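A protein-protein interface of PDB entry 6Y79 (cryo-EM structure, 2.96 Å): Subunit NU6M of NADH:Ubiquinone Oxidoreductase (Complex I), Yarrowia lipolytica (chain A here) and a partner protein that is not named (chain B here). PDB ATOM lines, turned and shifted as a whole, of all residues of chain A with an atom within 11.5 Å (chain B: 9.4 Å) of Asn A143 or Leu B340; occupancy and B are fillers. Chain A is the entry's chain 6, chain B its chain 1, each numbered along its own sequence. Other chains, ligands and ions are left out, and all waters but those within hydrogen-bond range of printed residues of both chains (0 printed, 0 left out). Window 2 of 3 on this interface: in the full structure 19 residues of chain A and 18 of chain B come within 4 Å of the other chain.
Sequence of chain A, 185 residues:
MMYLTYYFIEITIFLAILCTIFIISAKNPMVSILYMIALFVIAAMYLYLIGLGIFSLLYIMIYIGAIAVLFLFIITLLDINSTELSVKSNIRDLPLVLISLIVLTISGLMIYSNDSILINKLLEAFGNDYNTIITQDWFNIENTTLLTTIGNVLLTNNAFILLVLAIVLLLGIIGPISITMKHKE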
ATOM      1  N   ILE A  54      17.004 -17.682 -21.970  1.00  0.00           N
ATOM      2  CA  ILE A  54      16.939 -19.134 -21.818  1.00  0.00           C
ATOM      3  C   ILE A  54      16.242 -19.764 -23.019  1.00  0.00           C
ATOM      4  O   ILE A  54      16.718 -20.755 -23.599  1.00  0.00           O
ATOM      5  CB  ILE A  54      16.214 -19.495 -20.507  1.00  0.00           C
ATOM      6  CG1 ILE A  54      16.933 -18.926 -19.280  1.00  0.00           C
ATOM      7  CG2 ILE A  54      16.107 -20.991 -20.361  1.00  0.00           C
ATOM      8  CD1 ILE A  54      16.291 -17.707 -18.653  1.00  0.00           C
ATOM      9  N   PHE A 139      13.319  -7.822  -2.682  1.00  0.00           N
ATOM     10  CA  PHE A 139      12.614  -8.848  -1.922  1.00  0.00           C
ATOM     11  C   PHE A 139      13.075 -10.270  -2.216  1.00  0.00           C
ATOM     12  O   PHE A 139      12.669 -11.186  -1.498  1.00  0.00           O
ATOM     13  CB  PHE A 139      11.109  -8.775  -2.185  1.00  0.00           C
ATOM     14  CG  PHE A 139      10.449  -7.546  -1.645  1.00  0.00           C
ATOM     15  CD1 PHE A 139      10.244  -7.390  -0.287  1.00  0.00           C
ATOM     16  CD2 PHE A 139       9.996  -6.565  -2.506  1.00  0.00           C
ATOM     17  CE1 PHE A 139       9.618  -6.261   0.201  1.00  0.00           C
ATOM     18  CE2 PHE A 139       9.372  -5.439  -2.027  1.00  0.00           C
ATOM     19  CZ  PHE A 139       9.178  -5.289  -0.673  1.00  0.00           C
ATOM     20  N   ASN A 140      13.895 -10.487  -3.240  1.00  0.00           N
ATOM     21  CA  ASN A 140      14.275 -11.828  -3.675  1.00  0.00           C
ATOM     22  C   ASN A 140      15.747 -12.080  -3.384  1.00  0.00           C
ATOM     23  O   ASN A 140      16.608 -11.337  -3.853  1.00  0.00           O
ATOM     24  CB  ASN A 140      14.005 -12.006  -5.167  1.00  0.00           C
ATOM     25  CG  ASN A 140      14.206 -13.430  -5.627  1.00  0.00           C
ATOM     26  OD1 ASN A 140      14.200 -14.365  -4.828  1.00  0.00           O
ATOM     27  ND2 ASN A 140      14.401 -13.603  -6.925  1.00  0.00           N
ATOM     28  N   ILE A 141      16.036 -13.159  -2.662  1.00  0.00           N
ATOM     29  CA  ILE A 141      17.351 -13.382  -2.076  1.00  0.00           C
ATOM     30  C   ILE A 141      18.176 -14.423  -2.808  1.00  0.00           C
ATOM     31  O   ILE A 141      19.314 -14.678  -2.394  1.00  0.00           O
ATOM     32  CB  ILE A 141      17.230 -13.762  -0.590  1.00  0.00           C
ATOM     33  CG1 ILE A 141      16.173 -14.847  -0.429  1.00  0.00           C
ATOM     34  CG2 ILE A 141      16.869 -12.571   0.214  1.00  0.00           C
ATOM     35  CD1 ILE A 141      15.916 -15.260   0.981  1.00  0.00           C
ATOM     36  N   GLU A 142      17.667 -15.034  -3.874  1.00  0.00           N
ATOM     37  CA  GLU A 142      18.422 -16.132  -4.460  1.00  0.00           C
ATOM     38  C   GLU A 142      18.237 -16.207  -5.966  1.00  0.00           C
ATOM     39  O   GLU A 142      17.343 -15.583  -6.539  1.00  0.00           O
ATOM     40  CB  GLU A 142      18.036 -17.460  -3.834  1.00  0.00           C
ATOM     41  CG  GLU A 142      16.566 -17.709  -3.801  1.00  0.00           C
ATOM     42  CD  GLU A 142      16.264 -19.064  -3.229  1.00  0.00           C
ATOM     43  OE1 GLU A 142      17.180 -19.665  -2.630  1.00  0.00           O
ATOM     44  OE2 GLU A 142      15.123 -19.538  -3.388  1.00  0.00           O
ATOM     45  N   ASN A 143      19.096 -17.009  -6.597  1.00  0.00           N
ATOM     46  CA  ASN A 143      19.183 -17.082  -8.053  1.00  0.00           C
ATOM     47  C   ASN A 143      18.169 -18.089  -8.589  1.00  0.00           C
ATOM     48  O   ASN A 143      18.493 -19.075  -9.252  1.00  0.00           O
ATOM     49  CB  ASN A 143      20.601 -17.435  -8.481  1.00  0.00           C
ATOM     50  CG  ASN A 143      20.952 -16.885  -9.850  1.00  0.00           C
ATOM     51  OD1 ASN A 143      20.224 -16.068 -10.413  1.00  0.00           O
ATOM     52  ND2 ASN A 143      22.082 -17.327 -10.388  1.00  0.00           N
ATOM     53  N   THR A 144      16.910 -17.823  -8.280  1.00  0.00           N
ATOM     54  CA  THR A 144      15.833 -18.513  -8.964  1.00  0.00           C
ATOM     55  C   THR A 144      15.634 -17.816 -10.295  1.00  0.00           C
ATOM     56  O   THR A 144      14.967 -16.785 -10.380  1.00  0.00           O
ATOM     57  CB  THR A 144      14.561 -18.509  -8.133  1.00  0.00           C
ATOM     58  OG1 THR A 144      14.839 -19.040  -6.835  1.00  0.00           O
ATOM     59  CG2 THR A 144      13.541 -19.389  -8.798  1.00  0.00           C
ATOM     60  N   THR A 145      16.245 -18.356 -11.336  1.00  0.00           N
ATOM     61  CA  THR A 145      15.946 -17.878 -12.668  1.00  0.00           C
ATOM     62  C   THR A 145      14.753 -18.648 -13.216  1.00  0.00           C
ATOM     63  O   THR A 145      14.081 -19.397 -12.506  1.00  0.00           O
ATOM     64  CB  THR A 145      17.166 -17.998 -13.577  1.00  0.00           C
ATOM     65  OG1 THR A 145      17.507 -19.377 -13.755  1.00  0.00           O
ATOM     66  CG2 THR A 145      18.338 -17.258 -12.974  1.00  0.00           C
ATOM     67  N   LEU A 146      14.499 -18.467 -14.504  1.00  0.00           N
ATOM     68  CA  LEU A 146      13.242 -18.907 -15.090  1.00  0.00           C
ATOM     69  C   LEU A 146      13.193 -20.422 -15.258  1.00  0.00           C
ATOM     70  O   LEU A 146      12.128 -21.036 -15.106  1.00  0.00           O
ATOM     71  CB  LEU A 146      13.056 -18.184 -16.418  1.00  0.00           C
ATOM     72  CG  LEU A 146      11.829 -18.405 -17.273  1.00  0.00           C
ATOM     73  CD1 LEU A 146      11.404 -17.086 -17.822  1.00  0.00           C
ATOM     74  CD2 LEU A 146      12.230 -19.304 -18.388  1.00  0.00           C
ATOM     75  N   LEU A 147      14.335 -21.038 -15.565  1.00  0.00           N
ATOM     76  CA  LEU A 147      14.390 -22.487 -15.717  1.00  0.00           C
ATOM     77  C   LEU A 147      14.183 -23.197 -14.384  1.00  0.00           C
ATOM     78  O   LEU A 147      13.613 -24.293 -14.346  1.00  0.00           O
ATOM     79  CB  LEU A 147      15.725 -22.876 -16.344  1.00  0.00           C
ATOM     80  CG  LEU A 147      15.892 -24.305 -16.843  1.00  0.00           C
ATOM     81  CD1 LEU A 147      14.868 -24.611 -17.907  1.00  0.00           C
ATOM     82  CD2 LEU A 147      17.286 -24.489 -17.385  1.00  0.00           C
ATOM     83  N   THR A 148      14.588 -22.560 -13.285  1.00  0.00           N
ATOM     84  CA  THR A 148      14.335 -23.103 -11.958  1.00  0.00           C
ATOM     85  C   THR A 148      12.848 -23.120 -11.631  1.00  0.00           C
ATOM     86  O   THR A 148      12.337 -24.105 -11.087  1.00  0.00           O
ATOM     87  CB  THR A 148      15.100 -22.292 -10.918  1.00  0.00           C
ATOM     88  OG1 THR A 148      16.499 -22.341 -11.215  1.00  0.00           O
ATOM     89  CG2 THR A 148      14.870 -22.851  -9.530  1.00  0.00           C
ATOM     90  N   THR A 149      12.123 -22.055 -11.976  1.00  0.00           N
ATOM     91  CA  THR A 149      10.707 -22.031 -11.644  1.00  0.00           C
ATOM     92  C   THR A 149       9.908 -22.926 -12.582  1.00  0.00           C
ATOM     93  O   THR A 149       8.901 -23.511 -12.161  1.00  0.00           O
ATOM     94  CB  THR A 149      10.184 -20.600 -11.670  1.00  0.00           C
ATOM     95  OG1 THR A 149      11.125 -19.759 -11.005  1.00  0.00           O
ATOM     96  CG2 THR A 149       8.844 -20.526 -10.937  1.00  0.00           C
ATOM     97  N   ILE A 150      10.355 -23.080 -13.836  1.00  0.00           N
ATOM     98  CA  ILE A 150       9.748 -24.082 -14.712  1.00  0.00           C
ATOM     99  C   ILE A 150       9.958 -25.479 -14.142  1.00  0.00           C
ATOM    100  O   ILE A 150       9.039 -26.305 -14.126  1.00  0.00           O
ATOM    101  CB  ILE A 150      10.294 -23.960 -16.149  1.00  0.00           C
ATOM    102  CG1 ILE A 150       9.795 -22.675 -16.795  1.00  0.00           C
ATOM    103  CG2 ILE A 150       9.824 -25.109 -17.007  1.00  0.00           C
ATOM    104  CD1 ILE A 150      10.301 -22.469 -18.197  1.00  0.00           C
ATOM    105  N   GLY A 151      11.141 -25.743 -13.598  1.00  0.00           N
ATOM    106  CA  GLY A 151      11.348 -27.005 -12.922  1.00  0.00           C
ATOM    107  C   GLY A 151      10.641 -27.150 -11.589  1.00  0.00           C
ATOM    108  O   GLY A 151      10.513 -28.278 -11.112  1.00  0.00           O
ATOM    109  N   ASN A 152      10.226 -26.061 -10.952  1.00  0.00           N
ATOM    110  CA  ASN A 152       9.439 -26.222  -9.735  1.00  0.00           C
ATOM    111  C   ASN A 152       7.990 -26.514 -10.055  1.00  0.00           C
ATOM    112  O   ASN A 152       7.366 -27.334  -9.384  1.00  0.00           O
ATOM    113  CB  ASN A 152       9.521 -24.963  -8.860  1.00  0.00           C
ATOM    114  CG  ASN A 152       8.998 -25.168  -7.435  1.00  0.00           C
ATOM    115  OD1 ASN A 152       8.614 -26.269  -7.037  1.00  0.00           O
ATOM    116  ND2 ASN A 152       8.940 -24.080  -6.670  1.00  0.00           N
ATOM    117  N   LEU B 102      28.337 -15.580 -19.269  1.00  0.00           N
ATOM    118  CA  LEU B 102      26.897 -15.698 -19.202  1.00  0.00           C
ATOM    119  C   LEU B 102      26.559 -16.869 -18.292  1.00  0.00           C
ATOM    120  O   LEU B 102      27.266 -17.879 -18.268  1.00  0.00           O
ATOM    121  CB  LEU B 102      26.285 -15.845 -20.618  1.00  0.00           C
ATOM    122  CG  LEU B 102      26.619 -16.977 -21.592  1.00  0.00           C
ATOM    123  CD1 LEU B 102      25.569 -18.027 -21.528  1.00  0.00           C
ATOM    124  CD2 LEU B 102      26.705 -16.476 -23.005  1.00  0.00           C
ATOM    125  N   ASN B 103      25.474 -16.714 -17.526  1.00  0.00           N
ATOM    126  CA  ASN B 103      25.054 -17.650 -16.491  1.00  0.00           C
ATOM    127  C   ASN B 103      24.424 -18.920 -17.061  1.00  0.00           C
ATOM    128  O   ASN B 103      24.004 -19.771 -16.282  1.00  0.00           O
ATOM    129  CB  ASN B 103      24.065 -16.938 -15.561  1.00  0.00           C
ATOM    130  CG  ASN B 103      23.995 -17.537 -14.160  1.00  0.00           C
ATOM    131  OD1 ASN B 103      24.718 -18.472 -13.824  1.00  0.00           O
ATOM    132  ND2 ASN B 103      23.095 -16.996 -13.331  1.00  0.00           N
ATOM    133  N   LEU B 104      24.385 -19.110 -18.379  1.00  0.00           N
ATOM    134  CA  LEU B 104      23.773 -20.294 -18.976  1.00  0.00           C
ATOM    135  C   LEU B 104      24.738 -20.980 -19.922  1.00  0.00           C
ATOM    136  O   LEU B 104      24.335 -21.463 -20.984  1.00  0.00           O
ATOM    137  CB  LEU B 104      22.503 -19.939 -19.734  1.00  0.00           C
ATOM    138  CG  LEU B 104      21.330 -19.329 -18.987  1.00  0.00           C
ATOM    139  CD1 LEU B 104      20.449 -18.833 -20.075  1.00  0.00           C
ATOM    140  CD2 LEU B 104      20.600 -20.332 -18.103  1.00  0.00           C
ATOM    141  N   ILE B 158      25.409 -31.943 -14.330  1.00  0.00           N
ATOM    142  CA  ILE B 158      24.711 -30.792 -13.747  1.00  0.00           C
ATOM    143  C   ILE B 158      23.788 -31.177 -12.588  1.00  0.00           C
ATOM    144  O   ILE B 158      23.383 -30.311 -11.807  1.00  0.00           O
ATOM    145  CB  ILE B 158      24.031 -30.057 -14.928  1.00  0.00           C
ATOM    146  CG1 ILE B 158      25.101 -29.571 -15.892  1.00  0.00           C
ATOM    147  CG2 ILE B 158      23.255 -28.808 -14.546  1.00  0.00           C
ATOM    148  CD1 ILE B 158      24.563 -29.253 -17.239  1.00  0.00           C
ATOM    149  N   PHE B 160      24.926 -32.463 -10.005  1.00  0.00           N
ATOM    150  CA  PHE B 160      25.763 -32.205  -8.843  1.00  0.00           C
ATOM    151  C   PHE B 160      25.954 -30.734  -8.548  1.00  0.00           C
ATOM    152  O   PHE B 160      26.328 -30.390  -7.426  1.00  0.00           O
ATOM    153  CB  PHE B 160      27.150 -32.805  -9.040  1.00  0.00           C
ATOM    154  CG  PHE B 160      27.172 -34.283  -9.027  1.00  0.00           C
ATOM    155  CD1 PHE B 160      26.201 -34.997  -8.363  1.00  0.00           C
ATOM    156  CD2 PHE B 160      28.167 -34.964  -9.683  1.00  0.00           C
ATOM    157  CE1 PHE B 160      26.226 -36.362  -8.355  1.00  0.00           C
ATOM    158  CE2 PHE B 160      28.196 -36.329  -9.676  1.00  0.00           C
ATOM    159  CZ  PHE B 160      27.222 -37.028  -9.012  1.00  0.00           C
ATOM    160  N   VAL B 161      25.764 -29.871  -9.535  1.00  0.00           N
ATOM    161  CA  VAL B 161      26.016 -28.452  -9.388  1.00  0.00           C
ATOM    162  C   VAL B 161      24.719 -27.657  -9.342  1.00  0.00           C
ATOM    163  O   VAL B 161      24.605 -26.706  -8.567  1.00  0.00           O
ATOM    164  CB  VAL B 161      26.930 -27.951 -10.524  1.00  0.00           C
ATOM    165  CG1 VAL B 161      27.512 -26.574 -10.186  1.00  0.00           C
ATOM    166  CG2 VAL B 161      28.000 -28.990 -10.844  1.00  0.00           C
ATOM    167  N   SER B 162      23.729 -28.065 -10.144  1.00  0.00           N
ATOM    168  CA  SER B 162      22.466 -27.349 -10.349  1.00  0.00           C
ATOM    169  C   SER B 162      22.702 -25.902 -10.771  1.00  0.00           C
ATOM    170  O   SER B 162      22.067 -24.977 -10.271  1.00  0.00           O
ATOM    171  CB  SER B 162      21.566 -27.417  -9.116  1.00  0.00           C
ATOM    172  OG  SER B 162      20.379 -26.677  -9.313  1.00  0.00           O
ATOM    173  N   SER B 163      23.637 -25.699 -11.692  1.00  0.00           N
ATOM    174  CA  SER B 163      23.856 -24.381 -12.272  1.00  0.00           C
ATOM    175  C   SER B 163      24.421 -24.564 -13.663  1.00  0.00           C
ATOM    176  O   SER B 163      25.354 -25.343 -13.849  1.00  0.00           O
ATOM    177  CB  SER B 163      24.813 -23.529 -11.454  1.00  0.00           C
ATOM    178  OG  SER B 163      26.127 -23.917 -11.680  1.00  0.00           O
ATOM    179  N   LEU B 164      23.866 -23.840 -14.631  1.00  0.00           N
ATOM    180  CA  LEU B 164      24.352 -23.920 -15.997  1.00  0.00           C
ATOM    181  C   LEU B 164      25.545 -23.008 -16.257  1.00  0.00           C
ATOM    182  O   LEU B 164      26.043 -22.986 -17.383  1.00  0.00           O
ATOM    183  CB  LEU B 164      23.219 -23.611 -16.969  1.00  0.00           C
ATOM    184  CG  LEU B 164      22.136 -24.684 -17.071  1.00  0.00           C
ATOM    185  CD1 LEU B 164      21.104 -24.261 -18.071  1.00  0.00           C
ATOM    186  CD2 LEU B 164      22.720 -26.013 -17.465  1.00  0.00           C
ATOM    187  N   ASN B 165      26.004 -22.259 -15.259  1.00  0.00           N
ATOM    188  CA  ASN B 165      27.271 -21.555 -15.370  1.00  0.00           C
ATOM    189  C   ASN B 165      28.422 -22.552 -15.319  1.00  0.00           C
ATOM    190  O   ASN B 165      28.339 -23.588 -14.662  1.00  0.00           O
ATOM    191  CB  ASN B 165      27.406 -20.536 -14.244  1.00  0.00           C
ATOM    192  CG  ASN B 165      28.507 -19.547 -14.490  1.00  0.00           C
ATOM    193  OD1 ASN B 165      29.104 -19.523 -15.558  1.00  0.00           O
ATOM    194  ND2 ASN B 165      28.796 -18.733 -13.498  1.00  0.00           N
ATOM    195  N   THR B 168      31.216 -21.876 -12.325  1.00  0.00           N
ATOM    196  CA  THR B 168      30.604 -22.344 -11.090  1.00  0.00           C
ATOM    197  C   THR B 168      30.821 -23.841 -10.907  1.00  0.00           C
ATOM    198  O   THR B 168      31.072 -24.305  -9.789  1.00  0.00           O
ATOM    199  CB  THR B 168      29.118 -21.988 -11.092  1.00  0.00           C
ATOM    200  OG1 THR B 168      28.978 -20.572 -11.238  1.00  0.00           O
ATOM    201  CG2 THR B 168      28.453 -22.396  -9.797  1.00  0.00           C
ATOM    202  N   THR B 172      33.015 -25.579  -8.055  1.00  0.00           N
ATOM    203  CA  THR B 172      32.392 -26.675  -7.330  1.00  0.00           C
ATOM    204  C   THR B 172      33.295 -27.904  -7.292  1.00  0.00           C
ATOM    205  O   THR B 172      33.315 -28.635  -6.297  1.00  0.00           O
ATOM    206  CB  THR B 172      31.042 -26.967  -7.990  1.00  0.00           C
ATOM    207  OG1 THR B 172      30.250 -25.776  -7.962  1.00  0.00           O
ATOM    208  CG2 THR B 172      30.293 -28.025  -7.289  1.00  0.00           C
ATOM    209  N   PHE B 337      21.214 -32.600  -1.833  1.00  0.00           N
ATOM    210  CA  PHE B 337      20.806 -31.999  -3.063  1.00  0.00           C
ATOM    211  C   PHE B 337      21.558 -30.694  -3.232  1.00  0.00           C
ATOM    212  O   PHE B 337      21.714 -29.940  -2.266  1.00  0.00           O
ATOM    213  CB  PHE B 337      19.303 -31.726  -3.104  1.00  0.00           C
ATOM    214  CG  PHE B 337      18.454 -32.959  -3.136  1.00  0.00           C
ATOM    215  CD1 PHE B 337      18.323 -33.698  -4.292  1.00  0.00           C
ATOM    216  CD2 PHE B 337      17.773 -33.369  -2.007  1.00  0.00           C
ATOM    217  CE1 PHE B 337      17.535 -34.829  -4.324  1.00  0.00           C
ATOM    218  CE2 PHE B 337      16.987 -34.498  -2.033  1.00  0.00           C
ATOM    219  CZ  PHE B 337      16.870 -35.225  -3.193  1.00  0.00           C
ATOM    220  N   PRO B 338      22.064 -30.422  -4.423  1.00  0.00           N
ATOM    221  CA  PRO B 338      22.806 -29.182  -4.638  1.00  0.00           C
ATOM    222  C   PRO B 338      21.882 -27.985  -4.718  1.00  0.00           C
ATOM    223  O   PRO B 338      20.835 -28.020  -5.365  1.00  0.00           O
ATOM    224  CB  PRO B 338      23.511 -29.427  -5.972  1.00  0.00           C
ATOM    225  CG  PRO B 338      22.708 -30.453  -6.622  1.00  0.00           C
ATOM    226  CD  PRO B 338      22.164 -31.327  -5.573  1.00  0.00           C
ATOM    227  N   THR B 339      22.289 -26.914  -4.058  1.00  0.00           N
ATOM    228  CA  THR B 339      21.525 -25.683  -4.026  1.00  0.00           C
ATOM    229  C   THR B 339      22.059 -24.754  -5.110  1.00  0.00           C
ATOM    230  O   THR B 339      23.245 -24.804  -5.444  1.00  0.00           O
ATOM    231  CB  THR B 339      21.631 -25.046  -2.637  1.00  0.00           C
ATOM    232  OG1 THR B 339      21.427 -26.058  -1.649  1.00  0.00           O
ATOM    233  CG2 THR B 339      20.551 -23.985  -2.437  1.00  0.00           C
ATOM    234  N   LEU B 340      21.168 -23.950  -5.687  1.00  0.00           N
ATOM    235  CA  LEU B 340      21.519 -22.917  -6.656  1.00  0.00           C
ATOM    236  C   LEU B 340      22.560 -21.938  -6.132  1.00  0.00           C
ATOM    237  O   LEU B 340      23.474 -21.543  -6.855  1.00  0.00           O
ATOM    238  CB  LEU B 340      20.274 -22.135  -7.053  1.00  0.00           C
ATOM    239  CG  LEU B 340      19.192 -22.867  -7.823  1.00  0.00           C
ATOM    240  CD1 LEU B 340      17.933 -22.071  -7.674  1.00  0.00           C
ATOM    241  CD2 LEU B 340      19.576 -23.004  -9.277  1.00  0.00           C
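Hydrophobic or aromatic side chains of chain A that line the printed part of chain B: Ile A54 and Leu A147. Of the 16 printed residues of chain B, 4 touch a printed residue of chain A. Printed residues of chain B that touch a printed residue of chain A: Asn B103, Leu B104, Leu B164 and Leu B340. Among the printed residues, no Asp or Glu carboxylate lies within 4 Å of a Lys or Arg side-chain nitrogen of the other chain.
Leu B104 touches Ile A54. Leu B340 touches Asn A143 (CD1 to O, 3.4 Å). Leu A147 touches Leu B164 (CD2 to CD1, 3.9 Å). Thr A148 touches Leu B340.
The side-chain amide nitrogen of Asn B103 sits close to the side-chain amide nitrogen of Asn A143, 3.1 Å away.
The backbone carbonyl oxygen (O) of Asn B103 sits at hydrogen-bond distance from the backbone NH (N) of Asn B165, 3.4 Å away.
Asn A143 touches two residues of chain B. Thr A144 touches none of the printed residues of chain B. Of the printed residues of chain B, Leu A147 touches Leu B164. Of the printed residues of chain A, Asn B103 touches Asn A143 (3.1 Å). No residue of chain A comes within 4 Å of Ser B162. Of the printed residues of chain A, Leu B164 touches Leu A147 (3.9 Å). No residue of chain A comes within 4 Å of Pro B338. Thr B339 touches none of the printed residues of chain A. Leu B340 touches two residues of chain A. The nearest residue of chain A that does not touch Leu B340 is Thr A144 (4.3 Å).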
